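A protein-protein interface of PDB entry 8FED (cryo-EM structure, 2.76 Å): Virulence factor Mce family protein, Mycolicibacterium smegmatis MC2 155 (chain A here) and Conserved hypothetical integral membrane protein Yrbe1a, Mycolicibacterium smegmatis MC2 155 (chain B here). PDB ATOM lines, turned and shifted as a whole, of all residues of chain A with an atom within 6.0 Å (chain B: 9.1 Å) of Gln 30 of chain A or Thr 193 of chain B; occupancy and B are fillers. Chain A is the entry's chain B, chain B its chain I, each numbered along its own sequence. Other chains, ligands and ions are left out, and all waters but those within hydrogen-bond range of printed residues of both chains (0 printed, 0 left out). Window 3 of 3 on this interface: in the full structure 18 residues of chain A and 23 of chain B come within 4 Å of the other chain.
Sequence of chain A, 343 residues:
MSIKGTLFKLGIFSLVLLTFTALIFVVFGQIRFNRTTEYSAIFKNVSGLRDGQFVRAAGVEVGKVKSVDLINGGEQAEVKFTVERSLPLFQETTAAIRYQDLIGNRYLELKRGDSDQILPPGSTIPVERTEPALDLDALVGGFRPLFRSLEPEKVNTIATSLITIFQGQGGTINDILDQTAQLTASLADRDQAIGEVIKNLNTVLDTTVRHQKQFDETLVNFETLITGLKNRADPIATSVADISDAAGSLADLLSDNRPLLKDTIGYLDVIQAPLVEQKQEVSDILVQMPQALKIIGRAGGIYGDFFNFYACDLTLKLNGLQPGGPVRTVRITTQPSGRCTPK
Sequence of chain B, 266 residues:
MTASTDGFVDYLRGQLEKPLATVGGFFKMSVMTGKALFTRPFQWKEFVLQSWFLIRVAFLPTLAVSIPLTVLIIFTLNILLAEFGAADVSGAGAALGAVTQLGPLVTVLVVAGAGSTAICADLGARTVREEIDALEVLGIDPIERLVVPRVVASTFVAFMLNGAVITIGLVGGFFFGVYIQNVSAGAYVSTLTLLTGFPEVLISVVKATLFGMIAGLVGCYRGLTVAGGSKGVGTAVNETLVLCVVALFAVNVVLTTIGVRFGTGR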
ATOM      1  N   PHE A  25      22.151   1.504  21.197  1.00  0.00           N
ATOM      2  CA  PHE A  25      20.756   1.939  21.198  1.00  0.00           C
ATOM      3  C   PHE A  25      19.866   0.961  20.439  1.00  0.00           C
ATOM      4  O   PHE A  25      18.759   0.643  20.887  1.00  0.00           O
ATOM      5  CB  PHE A  25      20.638   3.343  20.606  1.00  0.00           C
ATOM      6  CG  PHE A  25      20.757   4.438  21.625  1.00  0.00           C
ATOM      7  CD1 PHE A  25      19.648   4.861  22.336  1.00  0.00           C
ATOM      8  CD2 PHE A  25      21.975   5.046  21.872  1.00  0.00           C
ATOM      9  CE1 PHE A  25      19.751   5.867  23.275  1.00  0.00           C
ATOM     10  CE2 PHE A  25      22.084   6.053  22.811  1.00  0.00           C
ATOM     11  CZ  PHE A  25      20.971   6.464  23.512  1.00  0.00           C
ATOM     12  N   VAL A  26      20.332   0.478  19.286  1.00  0.00           N
ATOM     13  CA  VAL A  26      19.557  -0.477  18.497  1.00  0.00           C
ATOM     14  C   VAL A  26      19.388  -1.789  19.255  1.00  0.00           C
ATOM     15  O   VAL A  26      18.296  -2.370  19.285  1.00  0.00           O
ATOM     16  CB  VAL A  26      20.219  -0.695  17.123  1.00  0.00           C
ATOM     17  CG1 VAL A  26      19.606  -1.887  16.412  1.00  0.00           C
ATOM     18  CG2 VAL A  26      20.085   0.554  16.270  1.00  0.00           C
ATOM     19  N   VAL A  27      20.461  -2.274  19.882  1.00  0.00           N
ATOM     20  CA  VAL A  27      20.413  -3.567  20.559  1.00  0.00           C
ATOM     21  C   VAL A  27      19.496  -3.508  21.774  1.00  0.00           C
ATOM     22  O   VAL A  27      18.650  -4.386  21.972  1.00  0.00           O
ATOM     23  CB  VAL A  27      21.835  -4.020  20.940  1.00  0.00           C
ATOM     24  CG1 VAL A  27      21.785  -5.113  21.988  1.00  0.00           C
ATOM     25  CG2 VAL A  27      22.576  -4.511  19.708  1.00  0.00           C
ATOM     26  N   PHE A  28      19.632  -2.472  22.596  1.00  0.00           N
ATOM     27  CA  PHE A  28      18.867  -2.404  23.833  1.00  0.00           C
ATOM     28  C   PHE A  28      17.542  -1.670  23.688  1.00  0.00           C
ATOM     29  O   PHE A  28      16.810  -1.547  24.675  1.00  0.00           O
ATOM     30  CB  PHE A  28      19.705  -1.751  24.934  1.00  0.00           C
ATOM     31  CG  PHE A  28      20.837  -2.610  25.411  1.00  0.00           C
ATOM     32  CD1 PHE A  28      20.588  -3.751  26.150  1.00  0.00           C
ATOM     33  CD2 PHE A  28      22.147  -2.284  25.115  1.00  0.00           C
ATOM     34  CE1 PHE A  28      21.620  -4.548  26.587  1.00  0.00           C
ATOM     35  CE2 PHE A  28      23.184  -3.079  25.551  1.00  0.00           C
ATOM     36  CZ  PHE A  28      22.918  -4.212  26.287  1.00  0.00           C
ATOM     37  N   GLY A  29      17.211  -1.186  22.495  1.00  0.00           N
ATOM     38  CA  GLY A  29      15.926  -0.553  22.277  1.00  0.00           C
ATOM     39  C   GLY A  29      15.016  -1.371  21.389  1.00  0.00           C
ATOM     40  O   GLY A  29      13.852  -1.007  21.184  1.00  0.00           O
ATOM     41  N   GLN A  30      15.542  -2.478  20.860  1.00  0.00           N
ATOM     42  CA  GLN A  30      14.813  -3.379  19.967  1.00  0.00           C
ATOM     43  C   GLN A  30      14.306  -2.628  18.734  1.00  0.00           C
ATOM     44  O   GLN A  30      13.106  -2.505  18.491  1.00  0.00           O
ATOM     45  CB  GLN A  30      13.666  -4.080  20.705  1.00  0.00           C
ATOM     46  CG  GLN A  30      14.056  -4.753  22.015  1.00  0.00           C
ATOM     47  CD  GLN A  30      14.661  -6.131  21.823  1.00  0.00           C
ATOM     48  OE1 GLN A  30      15.098  -6.488  20.729  1.00  0.00           O
ATOM     49  NE2 GLN A  30      14.684  -6.915  22.891  1.00  0.00           N
ATOM     50  N   ILE A  31      15.254  -2.119  17.955  1.00  0.00           N
ATOM     51  CA  ILE A  31      14.947  -1.351  16.754  1.00  0.00           C
ATOM     52  C   ILE A  31      14.947  -2.292  15.557  1.00  0.00           C
ATOM     53  O   ILE A  31      15.902  -3.049  15.348  1.00  0.00           O
ATOM     54  CB  ILE A  31      15.957  -0.207  16.560  1.00  0.00           C
ATOM     55  CG1 ILE A  31      15.962   0.712  17.781  1.00  0.00           C
ATOM     56  CG2 ILE A  31      15.624   0.590  15.313  1.00  0.00           C
ATOM     57  CD1 ILE A  31      14.642   1.400  18.034  1.00  0.00           C
ATOM     58  N   ARG A  32      13.874  -2.245  14.771  1.00  0.00           N
ATOM     59  CA  ARG A  32      13.735  -3.059  13.574  1.00  0.00           C
ATOM     60  C   ARG A  32      13.647  -2.166  12.345  1.00  0.00           C
ATOM     61  O   ARG A  32      13.152  -1.036  12.411  1.00  0.00           O
ATOM     62  CB  ARG A  32      12.495  -3.961  13.648  1.00  0.00           C
ATOM     63  CG  ARG A  32      12.774  -5.388  14.098  1.00  0.00           C
ATOM     64  CD  ARG A  32      13.327  -5.429  15.508  1.00  0.00           C
ATOM     65  NE  ARG A  32      13.586  -6.790  15.960  1.00  0.00           N
ATOM     66  CZ  ARG A  32      14.008  -7.104  17.177  1.00  0.00           C
ATOM     67  NH1 ARG A  32      14.230  -6.175  18.092  1.00  0.00           N
ATOM     68  NH2 ARG A  32      14.207  -8.381  17.486  1.00  0.00           N
ATOM     69  N   GLY A  52       5.527  -2.452  22.492  1.00  0.00           N
ATOM     70  CA  GLY A  52       6.884  -2.816  22.161  1.00  0.00           C
ATOM     71  C   GLY A  52       7.220  -4.278  22.341  1.00  0.00           C
ATOM     72  O   GLY A  52       8.323  -4.693  21.965  1.00  0.00           O
ATOM     73  N   PHE A  54       7.017  -8.253  21.420  1.00  0.00           N
ATOM     74  CA  PHE A  54       7.060  -8.855  20.095  1.00  0.00           C
ATOM     75  C   PHE A  54       5.717  -9.459  19.701  1.00  0.00           C
ATOM     76  O   PHE A  54       4.911  -9.857  20.545  1.00  0.00           O
ATOM     77  CB  PHE A  54       8.141  -9.932  20.034  1.00  0.00           C
ATOM     78  CG  PHE A  54       9.540  -9.395  20.112  1.00  0.00           C
ATOM     79  CD1 PHE A  54       9.809  -8.074  19.803  1.00  0.00           C
ATOM     80  CD2 PHE A  54      10.587 -10.215  20.493  1.00  0.00           C
ATOM     81  CE1 PHE A  54      11.094  -7.580  19.874  1.00  0.00           C
ATOM     82  CE2 PHE A  54      11.875  -9.724  20.566  1.00  0.00           C
ATOM     83  CZ  PHE A  54      12.127  -8.406  20.256  1.00  0.00           C
ATOM     84  N   LYS A  64       5.680  -6.217  16.069  1.00  0.00           N
ATOM     85  CA  LYS A  64       5.639  -5.728  17.438  1.00  0.00           C
ATOM     86  C   LYS A  64       4.225  -5.278  17.772  1.00  0.00           C
ATOM     87  O   LYS A  64       3.322  -5.313  16.933  1.00  0.00           O
ATOM     88  CB  LYS A  64       6.619  -4.572  17.652  1.00  0.00           C
ATOM     89  CG  LYS A  64       8.062  -4.979  17.800  1.00  0.00           C
ATOM     90  CD  LYS A  64       8.880  -3.778  18.212  1.00  0.00           C
ATOM     91  CE  LYS A  64      10.281  -4.165  18.607  1.00  0.00           C
ATOM     92  NZ  LYS A  64      10.984  -2.980  19.155  1.00  0.00           N
ATOM     93  N   GLY B  91      23.532 -13.009  31.510  1.00  0.00           N
ATOM     94  CA  GLY B  91      23.516 -11.917  30.551  1.00  0.00           C
ATOM     95  C   GLY B  91      22.743 -10.707  31.038  1.00  0.00           C
ATOM     96  O   GLY B  91      23.113  -9.569  30.747  1.00  0.00           O
ATOM     97  N   ALA B  92      21.658 -10.933  31.783  1.00  0.00           N
ATOM     98  CA  ALA B  92      20.857  -9.822  32.290  1.00  0.00           C
ATOM     99  C   ALA B  92      21.663  -8.951  33.244  1.00  0.00           C
ATOM    100  O   ALA B  92      21.732  -7.725  33.079  1.00  0.00           O
ATOM    101  CB  ALA B  92      19.601 -10.355  32.978  1.00  0.00           C
ATOM    102  N   GLY B  93      22.283  -9.571  34.249  1.00  0.00           N
ATOM    103  CA  GLY B  93      23.108  -8.816  35.176  1.00  0.00           C
ATOM    104  C   GLY B  93      24.317  -8.200  34.501  1.00  0.00           C
ATOM    105  O   GLY B  93      24.715  -7.080  34.825  1.00  0.00           O
ATOM    106  N   ALA B  94      24.911  -8.926  33.551  1.00  0.00           N
ATOM    107  CA  ALA B  94      26.042  -8.397  32.796  1.00  0.00           C
ATOM    108  C   ALA B  94      25.665  -7.115  32.067  1.00  0.00           C
ATOM    109  O   ALA B  94      26.355  -6.096  32.185  1.00  0.00           O
ATOM    110  CB  ALA B  94      26.534  -9.446  31.801  1.00  0.00           C
ATOM    111  N   ALA B  95      24.568  -7.152  31.308  1.00  0.00           N
ATOM    112  CA  ALA B  95      24.134  -5.980  30.558  1.00  0.00           C
ATOM    113  C   ALA B  95      23.764  -4.835  31.485  1.00  0.00           C
ATOM    114  O   ALA B  95      24.134  -3.683  31.232  1.00  0.00           O
ATOM    115  CB  ALA B  95      22.955  -6.340  29.658  1.00  0.00           C
ATOM    116  N   LEU B  96      23.043  -5.130  32.571  1.00  0.00           N
ATOM    117  CA  LEU B  96      22.647  -4.078  33.501  1.00  0.00           C
ATOM    118  C   LEU B  96      23.867  -3.391  34.101  1.00  0.00           C
ATOM    119  O   LEU B  96      23.982  -2.159  34.062  1.00  0.00           O
ATOM    120  CB  LEU B  96      21.756  -4.659  34.598  1.00  0.00           C
ATOM    121  CG  LEU B  96      21.155  -3.660  35.584  1.00  0.00           C
ATOM    122  CD1 LEU B  96      20.296  -2.643  34.856  1.00  0.00           C
ATOM    123  CD2 LEU B  96      20.345  -4.386  36.637  1.00  0.00           C
ATOM    124  N   VAL B  99      25.908  -1.378  31.444  1.00  0.00           N
ATOM    125  CA  VAL B  99      25.272  -0.192  30.885  1.00  0.00           C
ATOM    126  C   VAL B  99      25.126   0.898  31.936  1.00  0.00           C
ATOM    127  O   VAL B  99      25.540   2.043  31.719  1.00  0.00           O
ATOM    128  CB  VAL B  99      23.916  -0.559  30.255  1.00  0.00           C
ATOM    129  CG1 VAL B  99      23.115   0.692  29.955  1.00  0.00           C
ATOM    130  CG2 VAL B  99      24.131  -1.358  28.982  1.00  0.00           C
ATOM    131  N   LEU B 170      30.689  -5.485  27.098  1.00  0.00           N
ATOM    132  CA  LEU B 170      29.734  -6.545  26.781  1.00  0.00           C
ATOM    133  C   LEU B 170      30.363  -7.624  25.907  1.00  0.00           C
ATOM    134  O   LEU B 170      30.173  -8.822  26.156  1.00  0.00           O
ATOM    135  CB  LEU B 170      28.503  -5.959  26.094  1.00  0.00           C
ATOM    136  CG  LEU B 170      27.556  -5.145  26.972  1.00  0.00           C
ATOM    137  CD1 LEU B 170      26.408  -4.621  26.139  1.00  0.00           C
ATOM    138  CD2 LEU B 170      27.040  -5.984  28.122  1.00  0.00           C
ATOM    139  N   ALA B 187      22.141 -18.033  25.929  1.00  0.00           N
ATOM    140  CA  ALA B 187      21.625 -17.457  27.166  1.00  0.00           C
ATOM    141  C   ALA B 187      22.232 -16.094  27.451  1.00  0.00           C
ATOM    142  O   ALA B 187      21.575 -15.244  28.059  1.00  0.00           O
ATOM    143  CB  ALA B 187      21.866 -18.390  28.348  1.00  0.00           C
ATOM    144  N   TYR B 188      23.481 -15.871  27.042  1.00  0.00           N
ATOM    145  CA  TYR B 188      24.086 -14.562  27.248  1.00  0.00           C
ATOM    146  C   TYR B 188      23.440 -13.512  26.351  1.00  0.00           C
ATOM    147  O   TYR B 188      23.058 -12.436  26.821  1.00  0.00           O
ATOM    148  CB  TYR B 188      25.595 -14.626  27.003  1.00  0.00           C
ATOM    149  CG  TYR B 188      26.320 -13.353  27.381  1.00  0.00           C
ATOM    150  CD1 TYR B 188      26.498 -12.326  26.462  1.00  0.00           C
ATOM    151  CD2 TYR B 188      26.820 -13.174  28.663  1.00  0.00           C
ATOM    152  CE1 TYR B 188      27.151 -11.162  26.812  1.00  0.00           C
ATOM    153  CE2 TYR B 188      27.478 -12.014  29.019  1.00  0.00           C
ATOM    154  CZ  TYR B 188      27.642 -11.013  28.088  1.00  0.00           C
ATOM    155  OH  TYR B 188      28.295  -9.854  28.438  1.00  0.00           O
ATOM    156  N   VAL B 189      23.296 -13.811  25.058  1.00  0.00           N
ATOM    157  CA  VAL B 189      22.831 -12.772  24.141  1.00  0.00           C
ATOM    158  C   VAL B 189      21.327 -12.537  24.252  1.00  0.00           C
ATOM    159  O   VAL B 189      20.858 -11.416  24.031  1.00  0.00           O
ATOM    160  CB  VAL B 189      23.237 -13.102  22.695  1.00  0.00           C
ATOM    161  CG1 VAL B 189      24.744 -13.028  22.544  1.00  0.00           C
ATOM    162  CG2 VAL B 189      22.720 -14.469  22.286  1.00  0.00           C
ATOM    163  N   SER B 190      20.547 -13.563  24.591  1.00  0.00           N
ATOM    164  CA  SER B 190      19.099 -13.411  24.659  1.00  0.00           C
ATOM    165  C   SER B 190      18.611 -12.840  25.984  1.00  0.00           C
ATOM    166  O   SER B 190      17.423 -12.526  26.101  1.00  0.00           O
ATOM    167  CB  SER B 190      18.415 -14.753  24.406  1.00  0.00           C
ATOM    168  OG  SER B 190      18.918 -15.735  25.288  1.00  0.00           O
ATOM    169  N   THR B 191      19.484 -12.702  26.977  1.00  0.00           N
ATOM    170  CA  THR B 191      19.111 -12.125  28.260  1.00  0.00           C
ATOM    171  C   THR B 191      19.647 -10.716  28.458  1.00  0.00           C
ATOM    172  O   THR B 191      19.360 -10.108  29.493  1.00  0.00           O
ATOM    173  CB  THR B 191      19.586 -13.016  29.414  1.00  0.00           C
ATOM    174  OG1 THR B 191      20.929 -13.447  29.165  1.00  0.00           O
ATOM    175  CG2 THR B 191      18.687 -14.230  29.555  1.00  0.00           C
ATOM    176  N   LEU B 192      20.413 -10.184  27.501  1.00  0.00           N
ATOM    177  CA  LEU B 192      20.944  -8.832  27.644  1.00  0.00           C
ATOM    178  C   LEU B 192      19.822  -7.811  27.771  1.00  0.00           C
ATOM    179  O   LEU B 192      19.903  -6.885  28.584  1.00  0.00           O
ATOM    180  CB  LEU B 192      21.838  -8.485  26.452  1.00  0.00           C
ATOM    181  CG  LEU B 192      23.148  -9.250  26.269  1.00  0.00           C
ATOM    182  CD1 LEU B 192      23.874  -8.771  25.025  1.00  0.00           C
ATOM    183  CD2 LEU B 192      24.037  -9.111  27.488  1.00  0.00           C
ATOM    184  N   THR B 193      18.764  -7.970  26.984  1.00  0.00           N
ATOM    185  CA  THR B 193      17.647  -7.040  26.983  1.00  0.00           C
ATOM    186  C   THR B 193      16.616  -7.347  28.061  1.00  0.00           C
ATOM    187  O   THR B 193      15.601  -6.646  28.142  1.00  0.00           O
ATOM    188  CB  THR B 193      16.968  -7.040  25.612  1.00  0.00           C
ATOM    189  OG1 THR B 193      16.581  -8.376  25.271  1.00  0.00           O
ATOM    190  CG2 THR B 193      17.920  -6.513  24.551  1.00  0.00           C
ATOM    191  N   LEU B 194      16.841  -8.381  28.879  1.00  0.00           N
ATOM    192  CA  LEU B 194      15.870  -8.740  29.910  1.00  0.00           C
ATOM    193  C   LEU B 194      15.726  -7.638  30.951  1.00  0.00           C
ATOM    194  O   LEU B 194      14.609  -7.306  31.364  1.00  0.00           O
ATOM    195  CB  LEU B 194      16.274 -10.057  30.573  1.00  0.00           C
ATOM    196  CG  LEU B 194      15.418 -10.533  31.749  1.00  0.00           C
ATOM    197  CD1 LEU B 194      13.959 -10.659  31.347  1.00  0.00           C
ATOM    198  CD2 LEU B 194      15.941 -11.855  32.283  1.00  0.00           C
ATOM    199  N   LEU B 195      16.842  -7.056  31.387  1.00  0.00           N
ATOM    200  CA  LEU B 195      16.822  -6.015  32.402  1.00  0.00           C
ATOM    201  C   LEU B 195      17.341  -4.673  31.911  1.00  0.00           C
ATOM    202  O   LEU B 195      17.262  -3.692  32.657  1.00  0.00           O
ATOM    203  CB  LEU B 195      17.641  -6.443  33.630  1.00  0.00           C
ATOM    204  CG  LEU B 195      17.049  -7.552  34.502  1.00  0.00           C
ATOM    205  CD1 LEU B 195      18.010  -7.922  35.616  1.00  0.00           C
ATOM    206  CD2 LEU B 195      15.710  -7.123  35.075  1.00  0.00           C
ATOM    207  N   THR B 196      17.863  -4.598  30.691  1.00  0.00           N
ATOM    208  CA  THR B 196      18.403  -3.366  30.135  1.00  0.00           C
ATOM    209  C   THR B 196      17.537  -2.930  28.963  1.00  0.00           C
ATOM    210  O   THR B 196      17.277  -3.721  28.050  1.00  0.00           O
ATOM    211  CB  THR B 196      19.852  -3.555  29.681  1.00  0.00           C
ATOM    212  OG1 THR B 196      20.601  -4.188  30.724  1.00  0.00           O
ATOM    213  CG2 THR B 196      20.485  -2.215  29.363  1.00  0.00           C
ATOM    214  N   GLY B 197      17.097  -1.676  28.988  1.00  0.00           N
ATOM    215  CA  GLY B 197      16.268  -1.148  27.924  1.00  0.00           C
ATOM    216  C   GLY B 197      16.613   0.278  27.558  1.00  0.00           C
ATOM    217  O   GLY B 197      17.740   0.728  27.781  1.00  0.00           O
ATOM    218  N   PHE B 198      15.652   0.991  26.971  1.00  0.00           N
ATOM    219  CA  PHE B 198      15.870   2.399  26.650  1.00  0.00           C
ATOM    220  C   PHE B 198      16.146   3.278  27.869  1.00  0.00           C
ATOM    221  O   PHE B 198      17.028   4.150  27.765  1.00  0.00           O
ATOM    222  CB  PHE B 198      14.681   2.941  25.847  1.00  0.00           C
ATOM    223  CG  PHE B 198      15.050   3.418  24.475  1.00  0.00           C
ATOM    224  CD1 PHE B 198      15.661   4.649  24.298  1.00  0.00           C
ATOM    225  CD2 PHE B 198      14.793   2.637  23.361  1.00  0.00           C
ATOM    226  CE1 PHE B 198      16.005   5.091  23.036  1.00  0.00           C
ATOM    227  CE2 PHE B 198      15.134   3.073  22.097  1.00  0.00           C
ATOM    228  CZ  PHE B 198      15.741   4.302  21.934  1.00  0.00           C
ATOM    229  N   GLU B 200      17.764   2.588  30.552  1.00  0.00           N
ATOM    230  CA  GLU B 200      19.127   2.339  31.013  1.00  0.00           C
ATOM    231  C   GLU B 200      20.153   3.026  30.119  1.00  0.00           C
ATOM    232  O   GLU B 200      21.066   3.697  30.612  1.00  0.00           O
ATOM    233  CB  GLU B 200      19.394   0.836  31.084  1.00  0.00           C
ATOM    234  CG  GLU B 200      18.942   0.176  32.382  1.00  0.00           C
ATOM    235  CD  GLU B 200      17.446   0.272  32.609  1.00  0.00           C
ATOM    236  OE1 GLU B 200      16.689   0.230  31.619  1.00  0.00           O
ATOM    237  OE2 GLU B 200      17.026   0.395  33.778  1.00  0.00           O
ATOM    238  N   VAL B 201      20.025   2.872  28.799  1.00  0.00           N
ATOM    239  CA  VAL B 201      20.979   3.516  27.901  1.00  0.00           C
ATOM    240  C   VAL B 201      20.824   5.033  27.953  1.00  0.00           C
ATOM    241  O   VAL B 201      21.812   5.773  27.864  1.00  0.00           O
ATOM    242  CB  VAL B 201      20.845   2.967  26.468  1.00  0.00           C
ATOM    243  CG1 VAL B 201      21.306   1.524  26.416  1.00  0.00           C
ATOM    244  CG2 VAL B 201      19.424   3.077  25.966  1.00  0.00           C
ATOM    245  N   THR B 264      13.449  -0.568  34.144  1.00  0.00           N
ATOM    246  CA  THR B 264      12.893  -1.366  33.055  1.00  0.00           C
ATOM    247  C   THR B 264      11.939  -2.432  33.581  1.00  0.00           C
ATOM    248  O   THR B 264      10.856  -2.637  33.020  1.00  0.00           O
ATOM    249  CB  THR B 264      14.022  -2.005  32.245  1.00  0.00           C
ATOM    250  OG1 THR B 264      14.757  -0.985  31.560  1.00  0.00           O
ATOM    251  CG2 THR B 264      13.472  -2.989  31.224  1.00  0.00           C
ATOM    252  N   GLY B 265      12.315  -3.107  34.668  1.00  0.00           N
ATOM    253  CA  GLY B 265      11.486  -4.170  35.207  1.00  0.00           C
ATOM    254  C   GLY B 265      10.210  -3.692  35.864  1.00  0.00           C
ATOM    255  O   GLY B 265       9.265  -4.476  35.999  1.00  0.00           O
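Gly 29 of chain A touches just one residue of chain B: Phe 198 (3.6 Å).
Of chain B, only Thr 193 (3.4 Å) comes within 4 Å of Gln 30 of chain A.
No residue of chain B comes within 4 Å of Ile 31 of chain A.
Of the printed residues of chain A, Leu 192 of chain B touches Phe 28.
Of chain A, only Val 27 and Gln 30 come within 4 Å of Thr 193 of chain B.
Of the printed residues of chain A, Thr 196 of chain B touches Phe 28 (3.6 Å).
The nearest residue of chain B that does not touch Gln 30 of chain A is Phe 198 of chain B (5.7 Å).
The nearest residue of chain A that does not touch Thr 193 of chain B is Phe 28 of chain A (4.2 Å).
Hydrophobic or aromatic side chains of chain B within 4 Å of the printed part of chain A: Ala 95, Val 99, Leu 170, Leu 192, Phe 198 and Val 201.
Of the 11 printed residues of chain A, 5 touch a printed residue of chain B.
Hydrophobic or aromatic side chains of chain A that line the printed part of chain B: Phe 25 and Phe 28.
Among the printed residues, 13 pairs touch across the chains.
Among the printed residues, no Asp or Glu carboxylate lies within 4 Å of a Lys or Arg side-chain nitrogen of the other chain.
OH of Tyr 188 of chain B sits at hydrogen-bond distance from O of Leu 170 of chain B (3.1 Å).
The backbone NH (N) of Gly 197 of chain B sits at hydrogen-bond distance from the side-chain carboxylate (OE1) of Glu 200 of chain B (3.3 Å).
The guanidinium group of Arg 32 of chain A sits at hydrogen-bond distance from the side-chain amide oxygen of Gln 30 of chain A.
The backbone NH (N) of Leu 96 of chain B sits at hydrogen-bond distance from the side-chain hydroxyl (OG1) of Thr 196 of chain B.
Among the printed residues, merely in contact across the chains: Phe 25 of chain A with Phe 198 of chain B (3.7 Å), Phe 25 of chain A with Val 201 of chain B (3.9 Å), Val 27 of chain A with Thr 193 of chain B (3.4 Å), Phe 28 of chain A with Ala 95 of chain B (3.8 Å), Phe 28 of chain A with Val 99 of chain B (3.95 Å), Phe 28 of chain A with Leu 170 of chain B (3.5 Å), Phe 28 of chain A with Leu 192 of chain B (3.5 Å), Phe 28 of chain A with Thr 196 of chain B (3.6 Å), Phe 28 of chain A with Gly 197 of chain B (3.3 Å), Phe 28 of chain A with Phe 198 of chain B (3.6 Å), Phe 28 of chain A with Val 201 of chain B (3.9 Å) and Gly 29 of chain A with Phe 198 of chain B (3.6 Å).
OG1 of Thr 193 of chain B sits at hydrogen-bond distance from NE2 of Gln 30 of chain A (3.4 Å).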
